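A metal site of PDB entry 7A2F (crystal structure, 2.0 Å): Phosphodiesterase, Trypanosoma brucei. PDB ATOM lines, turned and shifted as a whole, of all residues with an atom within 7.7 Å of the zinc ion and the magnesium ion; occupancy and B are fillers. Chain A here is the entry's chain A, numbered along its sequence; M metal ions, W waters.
O of Leu 153 is in hydrogen-bond range of ND1 of His 187, at 2.7 Å.
ND1 of His 151 sits at hydrogen-bond distance from O of Ala 148 (2.7 Å).
A ring nitrogen (ND1) of His 115 lies within hydrogen-bond range of the side-chain hydroxyl (OH) of Tyr 110 (3.5 Å).
A ring nitrogen (NE2) of His 187 lies close to the backbone carbonyl oxygen of Leu 183 (3.4 Å).
N of His 115 is in hydrogen-bond range of OD1 of Asn 112 (3.3 Å).
OH of Tyr 105 sits at hydrogen-bond distance from N of Asp 152.
Water W2 is bound to the magnesium ion (1.9 Å).
OD1 of Asp 152 binds the magnesium ion, at 2.0 Å.
Water W5 is bound to the magnesium ion, at 2.1 Å.
The magnesium ion is bound by water W1, at 2.1 Å.
The magnesium ion is bound by water W3.
The magnesium ion is bound by water W4, at 2.3 Å.
Of the 24 residues printed, 4 come within 4 Å of the zinc ion.
The nearest printed residue that does not touch the zinc ion is His 111 (4.1 Å).
Water W6 is bound to the zinc ion (1.8 Å).
OD1 of Asp 264 is bound to the zinc ion, at 2.1 Å.
A ring nitrogen (NE2) of His 115 binds the zinc ion.
NE2 of His 151 binds the zinc ion (2.2 Å).
The zinc ion is bound by OD2 of Asp 152, 2.2 Å away.
Water W2 is bound to the zinc ion (2.4 Å).
The zinc ion has six donor atoms within binding distance.
His 187 touches the magnesium ion.
Of the 24 residues printed, 3 come within 4 Å of the magnesium ion.
Water W6 bridges a ring nitrogen (NE2) of His 111 (3.0 Å) and the side-chain carboxylate (OD2) of Asp 264 (3.1 Å).
Water W5 bridges OG1 of Thr 225 and O of His 151.
Water W4 lies within hydrogen-bond range of OE2 of Glu 184 (2.8 Å) and O of Thr 225 (3.0 Å).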
ATOM      1  N   TYR A 105       7.714  13.542 -25.504  1.00  0.00           N
ATOM      2  CA  TYR A 105       9.014  13.445 -24.773  1.00  0.00           C
ATOM      3  C   TYR A 105      10.114  13.940 -25.706  1.00  0.00           C
ATOM      4  O   TYR A 105       9.962  13.850 -26.918  1.00  0.00           O
ATOM      5  CB  TYR A 105       9.268  12.057 -24.192  1.00  0.00           C
ATOM      6  CG  TYR A 105       8.402  11.809 -22.994  1.00  0.00           C
ATOM      7  CD1 TYR A 105       8.753  12.331 -21.747  1.00  0.00           C
ATOM      8  CD2 TYR A 105       7.179  11.165 -23.129  1.00  0.00           C
ATOM      9  CE1 TYR A 105       7.909  12.169 -20.657  1.00  0.00           C
ATOM     10  CE2 TYR A 105       6.336  11.003 -22.039  1.00  0.00           C
ATOM     11  CZ  TYR A 105       6.703  11.516 -20.806  1.00  0.00           C
ATOM     12  OH  TYR A 105       5.853  11.336 -19.753  1.00  0.00           O
ATOM     13  N   TYR A 110      18.080  12.104 -19.690  1.00  0.00           N
ATOM     14  CA  TYR A 110      17.402  11.346 -18.607  1.00  0.00           C
ATOM     15  C   TYR A 110      15.861  11.412 -18.701  1.00  0.00           C
ATOM     16  O   TYR A 110      15.230  10.347 -18.836  1.00  0.00           O
ATOM     17  CB  TYR A 110      17.884  11.796 -17.225  1.00  0.00           C
ATOM     18  CG  TYR A 110      17.298  10.953 -16.114  1.00  0.00           C
ATOM     19  CD1 TYR A 110      17.812   9.704 -15.814  1.00  0.00           C
ATOM     20  CD2 TYR A 110      16.196  11.374 -15.391  1.00  0.00           C
ATOM     21  CE1 TYR A 110      17.260   8.918 -14.817  1.00  0.00           C
ATOM     22  CE2 TYR A 110      15.650  10.606 -14.380  1.00  0.00           C
ATOM     23  CZ  TYR A 110      16.172   9.358 -14.098  1.00  0.00           C
ATOM     24  OH  TYR A 110      15.652   8.600 -13.095  1.00  0.00           O
ATOM     25  N   HIS A 111      15.259  12.599 -18.626  1.00  0.00           N
ATOM     26  CA  HIS A 111      13.783  12.744 -18.587  1.00  0.00           C
ATOM     27  C   HIS A 111      13.199  12.630 -19.989  1.00  0.00           C
ATOM     28  O   HIS A 111      12.532  13.573 -20.452  1.00  0.00           O
ATOM     29  CB  HIS A 111      13.369  14.049 -17.922  1.00  0.00           C
ATOM     30  CG  HIS A 111      13.701  14.088 -16.486  1.00  0.00           C
ATOM     31  ND1 HIS A 111      14.797  14.755 -16.000  1.00  0.00           N
ATOM     32  CD2 HIS A 111      13.081  13.521 -15.432  1.00  0.00           C
ATOM     33  CE1 HIS A 111      14.834  14.601 -14.689  1.00  0.00           C
ATOM     34  NE2 HIS A 111      13.784  13.849 -14.307  1.00  0.00           N
ATOM     35  N   ASN A 112      13.414  11.479 -20.607  1.00  0.00           N
ATOM     36  CA  ASN A 112      12.931  11.149 -21.972  1.00  0.00           C
ATOM     37  C   ASN A 112      11.907  10.011 -21.839  1.00  0.00           C
ATOM     38  O   ASN A 112      11.561   9.650 -20.705  1.00  0.00           O
ATOM     39  CB  ASN A 112      14.115  10.786 -22.863  1.00  0.00           C
ATOM     40  CG  ASN A 112      14.945   9.660 -22.278  1.00  0.00           C
ATOM     41  OD1 ASN A 112      14.414   8.647 -21.834  1.00  0.00           O
ATOM     42  ND2 ASN A 112      16.251   9.867 -22.236  1.00  0.00           N
ATOM     43  N   HIS A 115      12.821   6.912 -19.567  1.00  0.00           N
ATOM     44  CA  HIS A 115      12.582   7.119 -18.112  1.00  0.00           C
ATOM     45  C   HIS A 115      11.123   6.783 -17.768  1.00  0.00           C
ATOM     46  O   HIS A 115      10.900   6.065 -16.758  1.00  0.00           O
ATOM     47  CB  HIS A 115      12.974   8.532 -17.675  1.00  0.00           C
ATOM     48  CG  HIS A 115      12.427   8.927 -16.342  1.00  0.00           C
ATOM     49  ND1 HIS A 115      12.845   8.338 -15.150  1.00  0.00           N
ATOM     50  CD2 HIS A 115      11.499   9.858 -16.000  1.00  0.00           C
ATOM     51  CE1 HIS A 115      12.200   8.906 -14.131  1.00  0.00           C
ATOM     52  NE2 HIS A 115      11.353   9.827 -14.635  1.00  0.00           N
ATOM     53  N   VAL A 116      10.141   7.244 -18.543  1.00  0.00           N
ATOM     54  CA  VAL A 116       8.718   7.092 -18.108  1.00  0.00           C
ATOM     55  C   VAL A 116       8.286   5.637 -18.345  1.00  0.00           C
ATOM     56  O   VAL A 116       7.554   5.095 -17.497  1.00  0.00           O
ATOM     57  CB  VAL A 116       7.767   8.133 -18.731  1.00  0.00           C
ATOM     58  CG1 VAL A 116       8.227   9.563 -18.416  1.00  0.00           C
ATOM     59  CG2 VAL A 116       7.555   7.974 -20.228  1.00  0.00           C
ATOM     60  N   VAL A 119       9.688   3.870 -15.351  1.00  0.00           N
ATOM     61  CA  VAL A 119       8.851   4.091 -14.129  1.00  0.00           C
ATOM     62  C   VAL A 119       7.595   3.215 -14.224  1.00  0.00           C
ATOM     63  O   VAL A 119       7.193   2.633 -13.214  1.00  0.00           O
ATOM     64  CB  VAL A 119       8.534   5.583 -13.939  1.00  0.00           C
ATOM     65  CG1 VAL A 119       7.488   5.829 -12.857  1.00  0.00           C
ATOM     66  CG2 VAL A 119       9.798   6.377 -13.657  1.00  0.00           C
ATOM     67  N   ALA A 148       2.378   6.853 -14.915  1.00  0.00           N
ATOM     68  CA  ALA A 148       3.840   6.720 -15.137  1.00  0.00           C
ATOM     69  C   ALA A 148       4.196   7.316 -16.499  1.00  0.00           C
ATOM     70  O   ALA A 148       5.237   7.981 -16.613  1.00  0.00           O
ATOM     71  CB  ALA A 148       4.257   5.286 -15.012  1.00  0.00           C
ATOM     72  N   HIS A 151       3.973  11.361 -16.630  1.00  0.00           N
ATOM     73  CA  HIS A 151       4.364  12.083 -15.398  1.00  0.00           C
ATOM     74  C   HIS A 151       5.496  13.086 -15.663  1.00  0.00           C
ATOM     75  O   HIS A 151       5.720  13.935 -14.768  1.00  0.00           O
ATOM     76  CB  HIS A 151       4.670  11.099 -14.255  1.00  0.00           C
ATOM     77  CG  HIS A 151       6.101  10.680 -14.207  1.00  0.00           C
ATOM     78  ND1 HIS A 151       6.565   9.597 -14.926  1.00  0.00           N
ATOM     79  CD2 HIS A 151       7.175  11.228 -13.594  1.00  0.00           C
ATOM     80  CE1 HIS A 151       7.861   9.484 -14.738  1.00  0.00           C
ATOM     81  NE2 HIS A 151       8.256  10.442 -13.913  1.00  0.00           N
ATOM     82  N   ASP A 152       6.170  13.027 -16.821  1.00  0.00           N
ATOM     83  CA  ASP A 152       7.249  13.997 -17.168  1.00  0.00           C
ATOM     84  C   ASP A 152       7.053  14.593 -18.576  1.00  0.00           C
ATOM     85  O   ASP A 152       8.048  15.077 -19.140  1.00  0.00           O
ATOM     86  CB  ASP A 152       8.632  13.317 -17.099  1.00  0.00           C
ATOM     87  CG  ASP A 152       9.257  13.299 -15.706  1.00  0.00           C
ATOM     88  OD1 ASP A 152       9.050  14.249 -14.918  1.00  0.00           O
ATOM     89  OD2 ASP A 152       9.970  12.316 -15.422  1.00  0.00           O
ATOM     90  N   LEU A 153       5.829  14.614 -19.099  1.00  0.00           N
ATOM     91  CA  LEU A 153       5.578  15.052 -20.508  1.00  0.00           C
ATOM     92  C   LEU A 153       6.272  16.390 -20.784  1.00  0.00           C
ATOM     93  O   LEU A 153       6.102  17.349 -20.000  1.00  0.00           O
ATOM     94  CB  LEU A 153       4.079  15.197 -20.777  1.00  0.00           C
ATOM     95  CG  LEU A 153       3.297  13.908 -20.926  1.00  0.00           C
ATOM     96  CD1 LEU A 153       1.811  14.218 -20.796  1.00  0.00           C
ATOM     97  CD2 LEU A 153       3.606  13.198 -22.240  1.00  0.00           C
ATOM     98  N   HIS A 155       9.327  17.378 -20.676  1.00  0.00           N
ATOM     99  CA  HIS A 155      10.522  17.731 -19.872  1.00  0.00           C
ATOM    100  C   HIS A 155      11.647  18.165 -20.819  1.00  0.00           C
ATOM    101  O   HIS A 155      11.881  17.458 -21.804  1.00  0.00           O
ATOM    102  CB  HIS A 155      10.961  16.539 -18.997  1.00  0.00           C
ATOM    103  CG  HIS A 155      11.679  16.929 -17.752  1.00  0.00           C
ATOM    104  ND1 HIS A 155      12.909  17.543 -17.780  1.00  0.00           N
ATOM    105  CD2 HIS A 155      11.327  16.819 -16.453  1.00  0.00           C
ATOM    106  CE1 HIS A 155      13.305  17.794 -16.547  1.00  0.00           C
ATOM    107  NE2 HIS A 155      12.337  17.341 -15.705  1.00  0.00           N
ATOM    108  N   ASN A 160      12.844  22.584 -11.809  1.00  0.00           N
ATOM    109  CA  ASN A 160      11.932  23.713 -11.450  1.00  0.00           C
ATOM    110  C   ASN A 160      12.786  24.936 -11.083  1.00  0.00           C
ATOM    111  O   ASN A 160      12.426  26.076 -11.493  1.00  0.00           O
ATOM    112  CB  ASN A 160      10.966  23.332 -10.316  1.00  0.00           C
ATOM    113  CG  ASN A 160       9.876  22.372 -10.758  1.00  0.00           C
ATOM    114  OD1 ASN A 160       9.659  22.194 -11.960  1.00  0.00           O
ATOM    115  ND2 ASN A 160       9.207  21.752  -9.796  1.00  0.00           N
ATOM    116  N   LEU A 183       7.249  22.268 -13.516  1.00  0.00           N
ATOM    117  CA  LEU A 183       7.189  21.170 -14.512  1.00  0.00           C
ATOM    118  C   LEU A 183       5.944  20.304 -14.293  1.00  0.00           C
ATOM    119  O   LEU A 183       5.301  19.926 -15.294  1.00  0.00           O
ATOM    120  CB  LEU A 183       8.469  20.332 -14.433  1.00  0.00           C
ATOM    121  CG  LEU A 183       9.694  21.021 -15.012  1.00  0.00           C
ATOM    122  CD1 LEU A 183      10.972  20.396 -14.493  1.00  0.00           C
ATOM    123  CD2 LEU A 183       9.664  21.007 -16.527  1.00  0.00           C
ATOM    124  N   GLU A 184       5.638  19.994 -13.026  1.00  0.00           N
ATOM    125  CA  GLU A 184       4.585  19.004 -12.691  1.00  0.00           C
ATOM    126  C   GLU A 184       3.251  19.539 -13.196  1.00  0.00           C
ATOM    127  O   GLU A 184       2.466  18.748 -13.775  1.00  0.00           O
ATOM    128  CB  GLU A 184       4.591  18.699 -11.191  1.00  0.00           C
ATOM    129  CG  GLU A 184       5.864  17.989 -10.744  1.00  0.00           C
ATOM    130  CD  GLU A 184       7.130  18.820 -10.580  1.00  0.00           C
ATOM    131  OE1 GLU A 184       7.053  20.050 -10.491  1.00  0.00           O
ATOM    132  OE2 GLU A 184       8.192  18.211 -10.525  1.00  0.00           O
ATOM    133  N   HIS A 187       3.268  19.093 -16.950  1.00  0.00           N
ATOM    134  CA  HIS A 187       3.044  17.668 -17.299  1.00  0.00           C
ATOM    135  C   HIS A 187       1.529  17.383 -17.255  1.00  0.00           C
ATOM    136  O   HIS A 187       1.020  16.756 -18.194  1.00  0.00           O
ATOM    137  CB  HIS A 187       3.831  16.685 -16.407  1.00  0.00           C
ATOM    138  CG  HIS A 187       5.304  16.968 -16.240  1.00  0.00           C
ATOM    139  ND1 HIS A 187       6.110  17.349 -17.293  1.00  0.00           N
ATOM    140  CD2 HIS A 187       6.085  16.934 -15.140  1.00  0.00           C
ATOM    141  CE1 HIS A 187       7.334  17.532 -16.837  1.00  0.00           C
ATOM    142  NE2 HIS A 187       7.346  17.278 -15.509  1.00  0.00           N
ATOM    143  N   VAL A 222       1.079  13.064 -10.178  1.00  0.00           N
ATOM    144  CA  VAL A 222       2.105  13.859 -10.910  1.00  0.00           C
ATOM    145  C   VAL A 222       2.561  15.022 -10.025  1.00  0.00           C
ATOM    146  O   VAL A 222       3.770  15.217  -9.918  1.00  0.00           O
ATOM    147  CB  VAL A 222       1.597  14.342 -12.281  1.00  0.00           C
ATOM    148  CG1 VAL A 222       2.619  15.234 -12.967  1.00  0.00           C
ATOM    149  CG2 VAL A 222       1.230  13.176 -13.170  1.00  0.00           C
ATOM    150  N   THR A 225       5.282  14.253  -7.464  1.00  0.00           N
ATOM    151  CA  THR A 225       6.655  13.925  -7.901  1.00  0.00           C
ATOM    152  C   THR A 225       7.605  15.127  -7.723  1.00  0.00           C
ATOM    153  O   THR A 225       8.824  14.929  -7.906  1.00  0.00           O
ATOM    154  CB  THR A 225       6.733  13.433  -9.356  1.00  0.00           C
ATOM    155  OG1 THR A 225       6.255  14.418 -10.270  1.00  0.00           O
ATOM    156  CG2 THR A 225       5.963  12.146  -9.555  1.00  0.00           C
ATOM    157  N   ASP A 226       7.106  16.313  -7.368  1.00  0.00           N
ATOM    158  CA  ASP A 226       7.965  17.490  -7.067  1.00  0.00           C
ATOM    159  C   ASP A 226       8.814  17.184  -5.816  1.00  0.00           C
ATOM    160  O   ASP A 226       8.226  17.044  -4.727  1.00  0.00           O
ATOM    161  CB  ASP A 226       7.118  18.759  -6.881  1.00  0.00           C
ATOM    162  CG  ASP A 226       7.955  20.021  -6.664  1.00  0.00           C
ATOM    163  OD1 ASP A 226       9.121  19.884  -6.339  1.00  0.00           O
ATOM    164  OD2 ASP A 226       7.410  21.111  -6.820  1.00  0.00           O
ATOM    165  N   MET A 227      10.145  17.101  -5.964  1.00  0.00           N
ATOM    166  CA  MET A 227      11.039  16.641  -4.853  1.00  0.00           C
ATOM    167  C   MET A 227      11.053  17.692  -3.715  1.00  0.00           C
ATOM    168  O   MET A 227      11.390  17.320  -2.583  1.00  0.00           O
ATOM    169  CB  MET A 227      12.452  16.325  -5.327  1.00  0.00           C
ATOM    170  CG  MET A 227      12.572  14.984  -6.053  1.00  0.00           C
ATOM    171  SD  MET A 227      12.062  13.581  -5.011  1.00  0.00           S
ATOM    172  CE  MET A 227      13.475  13.437  -3.910  1.00  0.00           C
ATOM    173  N   LEU A 260       4.168   6.252  -7.205  1.00  0.00           N
ATOM    174  CA  LEU A 260       4.754   6.997  -8.354  1.00  0.00           C
ATOM    175  C   LEU A 260       6.076   7.639  -7.908  1.00  0.00           C
ATOM    176  O   LEU A 260       7.040   7.565  -8.668  1.00  0.00           O
ATOM    177  CB  LEU A 260       3.802   8.064  -8.899  1.00  0.00           C
ATOM    178  CG  LEU A 260       4.363   8.881 -10.056  1.00  0.00           C
ATOM    179  CD1 LEU A 260       4.716   7.992 -11.249  1.00  0.00           C
ATOM    180  CD2 LEU A 260       3.393   9.961 -10.488  1.00  0.00           C
ATOM    181  N   GLY A 263       8.670   4.827  -7.877  1.00  0.00           N
ATOM    182  CA  GLY A 263       9.088   4.529  -9.253  1.00  0.00           C
ATOM    183  C   GLY A 263      10.035   5.594  -9.778  1.00  0.00           C
ATOM    184  O   GLY A 263      11.005   5.279 -10.512  1.00  0.00           O
ATOM    185  N   ASP A 264       9.765   6.833  -9.413  1.00  0.00           N
ATOM    186  CA  ASP A 264      10.513   7.996  -9.948  1.00  0.00           C
ATOM    187  C   ASP A 264      11.943   8.033  -9.360  1.00  0.00           C
ATOM    188  O   ASP A 264      12.830   8.501 -10.073  1.00  0.00           O
ATOM    189  CB  ASP A 264       9.792   9.313  -9.646  1.00  0.00           C
ATOM    190  CG  ASP A 264      10.105  10.381 -10.685  1.00  0.00           C
ATOM    191  OD1 ASP A 264      10.358  10.004 -11.833  1.00  0.00           O
ATOM    192  OD2 ASP A 264      10.053  11.584 -10.343  1.00  0.00           O
ATOM    193  N   ILE A 265      12.159   7.548  -8.124  1.00  0.00           N
ATOM    194  CA  ILE A 265      13.510   7.476  -7.500  1.00  0.00           C
ATOM    195  C   ILE A 265      13.985   6.010  -7.383  1.00  0.00           C
ATOM    196  O   ILE A 265      14.739   5.695  -6.430  1.00  0.00           O
ATOM    197  CB  ILE A 265      13.531   8.233  -6.152  1.00  0.00           C
ATOM    198  CG1 ILE A 265      12.605   7.625  -5.110  1.00  0.00           C
ATOM    199  CG2 ILE A 265      13.210   9.710  -6.363  1.00  0.00           C
ATOM    200  CD1 ILE A 265      12.800   8.214  -3.734  1.00  0.00           C
HETATM  201 ZN    ZN M   1      10.238  11.206 -13.519  1.00  0.00          ZN
HETATM  202 MG    MG M   2       9.189  14.776 -12.997  1.00  0.00          MG
HETATM  203  O   HOH W   1      11.325  14.721 -13.211  1.00  0.00           O
HETATM  204  O   HOH W   2       9.452  13.056 -12.240  1.00  0.00           O
HETATM  205  O   HOH W   3       9.230  16.851 -13.816  1.00  0.00           O
HETATM  206  O   HOH W   4       9.032  15.539 -10.859  1.00  0.00           O
HETATM  207  O   HOH W   5       7.121  14.805 -12.575  1.00  0.00           O
HETATM  208  O   HOH W   6      11.556  12.301 -12.955  1.00  0.00           O
